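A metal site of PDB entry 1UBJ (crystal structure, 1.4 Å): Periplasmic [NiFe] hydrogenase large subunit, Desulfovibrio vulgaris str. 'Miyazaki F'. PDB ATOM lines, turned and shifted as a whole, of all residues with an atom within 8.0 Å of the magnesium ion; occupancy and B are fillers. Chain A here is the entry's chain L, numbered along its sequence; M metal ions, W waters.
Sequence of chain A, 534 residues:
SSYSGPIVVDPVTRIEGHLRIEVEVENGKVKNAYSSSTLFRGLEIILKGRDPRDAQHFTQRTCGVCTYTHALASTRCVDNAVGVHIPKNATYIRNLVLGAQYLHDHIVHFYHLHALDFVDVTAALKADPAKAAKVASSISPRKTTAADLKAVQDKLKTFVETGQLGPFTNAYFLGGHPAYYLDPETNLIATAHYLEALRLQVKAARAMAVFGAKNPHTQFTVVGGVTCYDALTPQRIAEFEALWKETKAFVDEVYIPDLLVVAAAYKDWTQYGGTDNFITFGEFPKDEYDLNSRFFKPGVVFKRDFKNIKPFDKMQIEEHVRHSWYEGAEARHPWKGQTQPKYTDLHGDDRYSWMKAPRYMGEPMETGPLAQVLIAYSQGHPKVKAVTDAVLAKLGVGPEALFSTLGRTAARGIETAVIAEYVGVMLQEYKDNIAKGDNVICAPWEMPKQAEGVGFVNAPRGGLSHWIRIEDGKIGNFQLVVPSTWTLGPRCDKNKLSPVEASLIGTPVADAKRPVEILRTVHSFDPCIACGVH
The side-chain carboxylate (OE2) of Glu 44 lies close to the side-chain amide oxygen (OE1) of Gln 479, 3.3 Å away. OG1 of Thr 339 lies within hydrogen-bond range of OE1 of Glu 44, 2.8 Å away. The side-chain amino group of Lys 356 lies within salt-bridge range of the side-chain carboxylate of Glu 44 (3.96 Å). O of Cys 531 sits at hydrogen-bond distance from ND1 of His 534 (2.8 Å).
Of the 24 residues printed, 3 come within 4 Å of the magnesium ion. The nearest printed residue that does not touch the magnesium ion is Gln 479 (4.1 Å).
The magnesium ion is bound by water W2 (2.0 Å), water W1 (2.1 Å), water W3 (2.1 Å), O of Leu 480 (2.1 Å), NE2 of His 534 (2.2 Å) and OE2 of Glu 44 (2.2 Å). The magnesium ion has six donor atoms within binding distance.
Water W1 lies within hydrogen-bond range of OE1 of Glu 44 (2.6 Å) and NZ of Lys 356 (2.9 Å). Water W2 lies within hydrogen-bond range of the side-chain carboxylate (OE2) of Glu 319 (2.5 Å), the side-chain amide oxygen (OE1) of Gln 479 (2.7 Å) and the side-chain amino group (NZ) of Lys 356 (2.9 Å).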
ATOM      1  N   PHE A  40      20.279  20.006  30.695  1.00  0.00           N
ATOM      2  CA  PHE A  40      21.710  19.982  30.490  1.00  0.00           C
ATOM      3  C   PHE A  40      22.428  20.042  31.850  1.00  0.00           C
ATOM      4  O   PHE A  40      21.961  20.802  32.725  1.00  0.00           O
ATOM      5  CB  PHE A  40      22.130  21.192  29.667  1.00  0.00           C
ATOM      6  CG  PHE A  40      23.604  21.355  29.435  1.00  0.00           C
ATOM      7  CD1 PHE A  40      24.295  20.594  28.503  1.00  0.00           C
ATOM      8  CD2 PHE A  40      24.320  22.309  30.171  1.00  0.00           C
ATOM      9  CE1 PHE A  40      25.647  20.743  28.275  1.00  0.00           C
ATOM     10  CE2 PHE A  40      25.671  22.469  29.923  1.00  0.00           C
ATOM     11  CZ  PHE A  40      26.349  21.713  28.974  1.00  0.00           C
ATOM     12  N   GLU A  44      31.093  17.328  30.682  1.00  0.00           N
ATOM     13  CA  GLU A  44      32.319  17.540  29.911  1.00  0.00           C
ATOM     14  C   GLU A  44      33.014  18.848  30.287  1.00  0.00           C
ATOM     15  O   GLU A  44      34.254  18.918  30.291  1.00  0.00           O
ATOM     16  CB  GLU A  44      32.017  17.503  28.405  1.00  0.00           C
ATOM     17  CG  GLU A  44      31.548  16.121  27.947  1.00  0.00           C
ATOM     18  CD  GLU A  44      30.657  16.170  26.712  1.00  0.00           C
ATOM     19  OE1 GLU A  44      30.068  17.235  26.477  1.00  0.00           O
ATOM     20  OE2 GLU A  44      30.551  15.080  26.055  1.00  0.00           O
ATOM     21  N   GLU A 319      29.848  14.921  15.874  1.00  0.00           N
ATOM     22  CA  GLU A 319      28.638  15.367  16.584  1.00  0.00           C
ATOM     23  C   GLU A 319      28.218  16.777  16.133  1.00  0.00           C
ATOM     24  O   GLU A 319      28.957  17.745  16.292  1.00  0.00           O
ATOM     25  CB  GLU A 319      28.883  15.328  18.086  1.00  0.00           C
ATOM     26  CG  GLU A 319      29.126  13.891  18.603  1.00  0.00           C
ATOM     27  CD  GLU A 319      29.168  13.981  20.115  1.00  0.00           C
ATOM     28  OE1 GLU A 319      28.159  13.572  20.756  1.00  0.00           O
ATOM     29  OE2 GLU A 319      30.160  14.478  20.691  1.00  0.00           O
ATOM     30  N   TYR A 326      23.824  24.710  21.350  1.00  0.00           N
ATOM     31  CA  TYR A 326      25.242  24.984  21.515  1.00  0.00           C
ATOM     32  C   TYR A 326      25.650  26.052  20.512  1.00  0.00           C
ATOM     33  O   TYR A 326      24.946  26.356  19.542  1.00  0.00           O
ATOM     34  CB  TYR A 326      26.095  23.708  21.272  1.00  0.00           C
ATOM     35  CG  TYR A 326      25.731  22.658  22.299  1.00  0.00           C
ATOM     36  CD1 TYR A 326      24.849  21.620  21.991  1.00  0.00           C
ATOM     37  CD2 TYR A 326      26.256  22.707  23.586  1.00  0.00           C
ATOM     38  CE1 TYR A 326      24.494  20.662  22.930  1.00  0.00           C
ATOM     39  CE2 TYR A 326      25.906  21.757  24.535  1.00  0.00           C
ATOM     40  CZ  TYR A 326      25.045  20.724  24.212  1.00  0.00           C
ATOM     41  OH  TYR A 326      24.686  19.787  25.154  1.00  0.00           O
ATOM     42  N   PRO A 334      34.861  13.708  18.296  1.00  0.00           N
ATOM     43  CA  PRO A 334      34.976  13.900  19.749  1.00  0.00           C
ATOM     44  C   PRO A 334      36.405  14.149  20.228  1.00  0.00           C
ATOM     45  O   PRO A 334      36.522  14.741  21.309  1.00  0.00           O
ATOM     46  CB  PRO A 334      34.431  12.615  20.367  1.00  0.00           C
ATOM     47  CG  PRO A 334      33.960  11.760  19.290  1.00  0.00           C
ATOM     48  CD  PRO A 334      34.195  12.421  17.967  1.00  0.00           C
ATOM     49  N   GLY A 337      36.141  17.695  20.198  1.00  0.00           N
ATOM     50  CA  GLY A 337      34.791  18.092  20.555  1.00  0.00           C
ATOM     51  C   GLY A 337      34.736  19.423  21.292  1.00  0.00           C
ATOM     52  O   GLY A 337      35.727  19.889  21.856  1.00  0.00           O
ATOM     53  N   GLN A 338      33.529  20.006  21.254  1.00  0.00           N
ATOM     54  CA  GLN A 338      33.239  21.288  21.882  1.00  0.00           C
ATOM     55  C   GLN A 338      31.933  21.207  22.638  1.00  0.00           C
ATOM     56  O   GLN A 338      30.991  20.642  22.098  1.00  0.00           O
ATOM     57  CB  GLN A 338      33.140  22.457  20.867  1.00  0.00           C
ATOM     58  CG  GLN A 338      34.447  22.600  20.075  1.00  0.00           C
ATOM     59  CD  GLN A 338      34.353  23.820  19.154  1.00  0.00           C
ATOM     60  OE1 GLN A 338      35.076  24.815  19.298  1.00  0.00           O
ATOM     61  NE2 GLN A 338      33.441  23.666  18.206  1.00  0.00           N
ATOM     62  N   THR A 339      31.858  21.746  23.847  1.00  0.00           N
ATOM     63  CA  THR A 339      30.575  21.763  24.563  1.00  0.00           C
ATOM     64  C   THR A 339      30.360  23.178  25.093  1.00  0.00           C
ATOM     65  O   THR A 339      30.821  23.542  26.169  1.00  0.00           O
ATOM     66  CB  THR A 339      30.586  20.675  25.643  1.00  0.00           C
ATOM     67  OG1 THR A 339      30.919  19.431  25.008  1.00  0.00           O
ATOM     68  CG2 THR A 339      29.201  20.567  26.280  1.00  0.00           C
ATOM     69  N   TRP A 354      19.065  19.757  23.959  1.00  0.00           N
ATOM     70  CA  TRP A 354      20.398  19.806  24.588  1.00  0.00           C
ATOM     71  C   TRP A 354      21.263  18.652  24.126  1.00  0.00           C
ATOM     72  O   TRP A 354      22.454  18.601  24.418  1.00  0.00           O
ATOM     73  CB  TRP A 354      20.291  19.786  26.123  1.00  0.00           C
ATOM     74  CG  TRP A 354      19.848  21.119  26.664  1.00  0.00           C
ATOM     75  CD1 TRP A 354      18.635  21.386  27.240  1.00  0.00           C
ATOM     76  CD2 TRP A 354      20.579  22.363  26.680  1.00  0.00           C
ATOM     77  NE1 TRP A 354      18.584  22.717  27.618  1.00  0.00           N
ATOM     78  CE2 TRP A 354      19.762  23.333  27.284  1.00  0.00           C
ATOM     79  CE3 TRP A 354      21.858  22.736  26.237  1.00  0.00           C
ATOM     80  CZ2 TRP A 354      20.200  24.663  27.448  1.00  0.00           C
ATOM     81  CZ3 TRP A 354      22.305  24.031  26.397  1.00  0.00           C
ATOM     82  CH2 TRP A 354      21.451  24.982  27.006  1.00  0.00           C
ATOM     83  N   MET A 355      20.692  17.661  23.418  1.00  0.00           N
ATOM     84  CA  MET A 355      21.603  16.671  22.835  1.00  0.00           C
ATOM     85  C   MET A 355      22.266  17.161  21.554  1.00  0.00           C
ATOM     86  O   MET A 355      21.627  17.823  20.739  1.00  0.00           O
ATOM     87  CB  MET A 355      20.855  15.401  22.452  1.00  0.00           C
ATOM     88  CG  MET A 355      20.397  14.549  23.635  1.00  0.00           C
ATOM     89  SD  MET A 355      19.944  12.910  23.043  1.00  0.00           S
ATOM     90  CE  MET A 355      18.902  12.311  24.374  1.00  0.00           C
ATOM     91  N   LYS A 356      23.526  16.773  21.359  1.00  0.00           N
ATOM     92  CA  LYS A 356      24.216  16.865  20.057  1.00  0.00           C
ATOM     93  C   LYS A 356      23.658  15.796  19.137  1.00  0.00           C
ATOM     94  O   LYS A 356      22.911  14.924  19.651  1.00  0.00           O
ATOM     95  CB  LYS A 356      25.732  16.677  20.222  1.00  0.00           C
ATOM     96  CG  LYS A 356      26.347  17.758  21.141  1.00  0.00           C
ATOM     97  CD  LYS A 356      27.832  17.517  21.339  1.00  0.00           C
ATOM     98  CE  LYS A 356      28.524  18.542  22.249  1.00  0.00           C
ATOM     99  NZ  LYS A 356      29.927  18.043  22.600  1.00  0.00           N
ATOM    100  N   PRO A 358      24.931  13.029  16.781  1.00  0.00           N
ATOM    101  CA  PRO A 358      26.070  12.270  16.207  1.00  0.00           C
ATOM    102  C   PRO A 358      25.647  11.684  14.862  1.00  0.00           C
ATOM    103  O   PRO A 358      24.545  11.170  14.635  1.00  0.00           O
ATOM    104  CB  PRO A 358      26.312  11.181  17.259  1.00  0.00           C
ATOM    105  CG  PRO A 358      25.559  11.603  18.498  1.00  0.00           C
ATOM    106  CD  PRO A 358      24.345  12.325  17.949  1.00  0.00           C
ATOM    107  N   SER A 465      30.937   5.777  23.845  1.00  0.00           N
ATOM    108  CA  SER A 465      32.376   6.023  23.718  1.00  0.00           C
ATOM    109  C   SER A 465      32.717   7.300  24.523  1.00  0.00           C
ATOM    110  O   SER A 465      31.995   8.281  24.535  1.00  0.00           O
ATOM    111  CB  SER A 465      32.835   6.118  22.248  1.00  0.00           C
ATOM    112  OG  SER A 465      32.020   7.067  21.571  1.00  0.00           O
ATOM    113  N   TRP A 467      36.055   9.862  25.216  1.00  0.00           N
ATOM    114  CA  TRP A 467      37.234  10.288  24.449  1.00  0.00           C
ATOM    115  C   TRP A 467      38.035  11.257  25.302  1.00  0.00           C
ATOM    116  O   TRP A 467      37.469  12.251  25.742  1.00  0.00           O
ATOM    117  CB  TRP A 467      36.745  10.954  23.153  1.00  0.00           C
ATOM    118  CG  TRP A 467      35.826  10.108  22.312  1.00  0.00           C
ATOM    119  CD1 TRP A 467      34.502   9.802  22.514  1.00  0.00           C
ATOM    120  CD2 TRP A 467      36.233   9.430  21.107  1.00  0.00           C
ATOM    121  NE1 TRP A 467      34.078   8.985  21.491  1.00  0.00           N
ATOM    122  CE2 TRP A 467      35.115   8.753  20.616  1.00  0.00           C
ATOM    123  CE3 TRP A 467      37.446   9.362  20.391  1.00  0.00           C
ATOM    124  CZ2 TRP A 467      35.156   7.984  19.440  1.00  0.00           C
ATOM    125  CZ3 TRP A 467      37.497   8.611  19.234  1.00  0.00           C
ATOM    126  CH2 TRP A 467      36.348   7.944  18.782  1.00  0.00           C
ATOM    127  N   PHE A 478      37.486  16.155  27.367  1.00  0.00           N
ATOM    128  CA  PHE A 478      36.860  14.865  27.644  1.00  0.00           C
ATOM    129  C   PHE A 478      35.479  14.916  26.991  1.00  0.00           C
ATOM    130  O   PHE A 478      34.710  15.807  27.395  1.00  0.00           O
ATOM    131  CB  PHE A 478      36.782  14.563  29.143  1.00  0.00           C
ATOM    132  CG  PHE A 478      36.650  13.081  29.448  1.00  0.00           C
ATOM    133  CD1 PHE A 478      35.423  12.450  29.167  1.00  0.00           C
ATOM    134  CD2 PHE A 478      37.691  12.342  29.970  1.00  0.00           C
ATOM    135  CE1 PHE A 478      35.290  11.094  29.429  1.00  0.00           C
ATOM    136  CE2 PHE A 478      37.531  10.974  30.227  1.00  0.00           C
ATOM    137  CZ  PHE A 478      36.336  10.333  29.959  1.00  0.00           C
ATOM    138  N   GLN A 479      35.213  14.015  26.073  1.00  0.00           N
ATOM    139  CA  GLN A 479      33.925  14.025  25.368  1.00  0.00           C
ATOM    140  C   GLN A 479      33.271  12.650  25.501  1.00  0.00           C
ATOM    141  O   GLN A 479      33.914  11.600  25.286  1.00  0.00           O
ATOM    142  CB  GLN A 479      34.095  14.402  23.885  1.00  0.00           C
ATOM    143  CG  GLN A 479      34.621  15.820  23.699  1.00  0.00           C
ATOM    144  CD  GLN A 479      33.587  16.871  24.036  1.00  0.00           C
ATOM    145  OE1 GLN A 479      32.381  16.643  23.789  1.00  0.00           O
ATOM    146  NE2 GLN A 479      34.030  17.999  24.554  1.00  0.00           N
ATOM    147  N   LEU A 480      31.990  12.666  25.900  1.00  0.00           N
ATOM    148  CA  LEU A 480      31.144  11.491  25.892  1.00  0.00           C
ATOM    149  C   LEU A 480      30.205  11.514  24.675  1.00  0.00           C
ATOM    150  O   LEU A 480      29.663  12.542  24.418  1.00  0.00           O
ATOM    151  CB  LEU A 480      30.247  11.445  27.118  1.00  0.00           C
ATOM    152  CG  LEU A 480      30.813  11.606  28.517  1.00  0.00           C
ATOM    153  CD1 LEU A 480      29.804  11.029  29.535  1.00  0.00           C
ATOM    154  CD2 LEU A 480      32.112  10.920  28.631  1.00  0.00           C
ATOM    155  N   VAL A 481      30.096  10.372  23.985  1.00  0.00           N
ATOM    156  CA  VAL A 481      29.194  10.236  22.873  1.00  0.00           C
ATOM    157  C   VAL A 481      28.405   8.988  23.268  1.00  0.00           C
ATOM    158  O   VAL A 481      28.967   7.890  23.332  1.00  0.00           O
ATOM    159  CB  VAL A 481      29.876  10.047  21.511  1.00  0.00           C
ATOM    160  CG1 VAL A 481      28.804   9.977  20.408  1.00  0.00           C
ATOM    161  CG2 VAL A 481      30.866  11.166  21.240  1.00  0.00           C
ATOM    162  N   VAL A 482      27.126   9.183  23.607  1.00  0.00           N
ATOM    163  CA  VAL A 482      26.398   8.136  24.361  1.00  0.00           C
ATOM    164  C   VAL A 482      25.345   7.502  23.481  1.00  0.00           C
ATOM    165  O   VAL A 482      24.886   8.178  22.537  1.00  0.00           O
ATOM    166  CB  VAL A 482      25.867   8.823  25.623  1.00  0.00           C
ATOM    167  CG1 VAL A 482      25.238   7.891  26.600  1.00  0.00           C
ATOM    168  CG2 VAL A 482      26.987   9.541  26.393  1.00  0.00           C
ATOM    169  N   THR A 485      22.379   9.552  22.658  1.00  0.00           N
ATOM    170  CA  THR A 485      22.730  10.711  21.836  1.00  0.00           C
ATOM    171  C   THR A 485      22.567  10.355  20.361  1.00  0.00           C
ATOM    172  O   THR A 485      22.012  11.137  19.598  1.00  0.00           O
ATOM    173  CB  THR A 485      24.191  11.171  22.067  1.00  0.00           C
ATOM    174  OG1 THR A 485      24.551  11.073  23.449  1.00  0.00           O
ATOM    175  CG2 THR A 485      24.403  12.607  21.610  1.00  0.00           C
ATOM    176  N   CYS A 531      22.039  10.337  30.069  1.00  0.00           N
ATOM    177  CA  CYS A 531      23.046   9.769  29.167  1.00  0.00           C
ATOM    178  C   CYS A 531      23.236  10.602  27.916  1.00  0.00           C
ATOM    179  O   CYS A 531      24.329  10.973  27.510  1.00  0.00           O
ATOM    180  CB  CYS A 531      22.583   8.363  28.716  1.00  0.00           C
ATOM    181  SG  CYS A 531      23.293   7.111  29.835  1.00  0.00           S
ATOM    182  N   GLY A 532      22.097  10.879  27.249  1.00  0.00           N
ATOM    183  CA  GLY A 532      22.229  11.532  25.956  1.00  0.00           C
ATOM    184  C   GLY A 532      22.863  12.892  25.949  1.00  0.00           C
ATOM    185  O   GLY A 532      23.637  13.241  25.025  1.00  0.00           O
ATOM    186  N   VAL A 533      22.563  13.683  26.996  1.00  0.00           N
ATOM    187  CA  VAL A 533      23.038  15.053  27.074  1.00  0.00           C
ATOM    188  C   VAL A 533      24.234  15.252  27.976  1.00  0.00           C
ATOM    189  O   VAL A 533      25.170  16.009  27.650  1.00  0.00           O
ATOM    190  CB  VAL A 533      21.952  15.974  27.699  1.00  0.00           C
ATOM    191  CG1 VAL A 533      22.456  17.397  27.877  1.00  0.00           C
ATOM    192  CG2 VAL A 533      20.687  15.955  26.854  1.00  0.00           C
ATOM    193  N   HIS A 534      24.317  14.561  29.130  1.00  0.00           N
ATOM    194  CA  HIS A 534      25.403  14.658  30.120  1.00  0.00           C
ATOM    195  C   HIS A 534      25.787  16.121  30.376  1.00  0.00           C
ATOM    196  O   HIS A 534      24.771  16.977  30.552  1.00  0.00           O
ATOM    197  CB  HIS A 534      26.632  13.806  29.787  1.00  0.00           C
ATOM    198  CG  HIS A 534      27.038  13.718  28.346  1.00  0.00           C
ATOM    199  ND1 HIS A 534      26.317  12.913  27.468  1.00  0.00           N
ATOM    200  CD2 HIS A 534      27.942  14.382  27.591  1.00  0.00           C
ATOM    201  CE1 HIS A 534      26.816  13.057  26.249  1.00  0.00           C
ATOM    202  NE2 HIS A 534      27.771  13.934  26.306  1.00  0.00           N
ATOM    203  OXT HIS A 534      26.912  16.596  30.432  1.00  0.00           O
HETATM  204 MG    MG M   1      28.992  14.569  24.623  1.00  0.00          MG
HETATM  205  O   HOH W   1      28.399  16.550  24.626  1.00  0.00           O
HETATM  206  O   HOH W   2      30.235  15.208  23.131  1.00  0.00           O
HETATM  207  O   HOH W   3      27.456  14.103  23.230  1.00  0.00           O
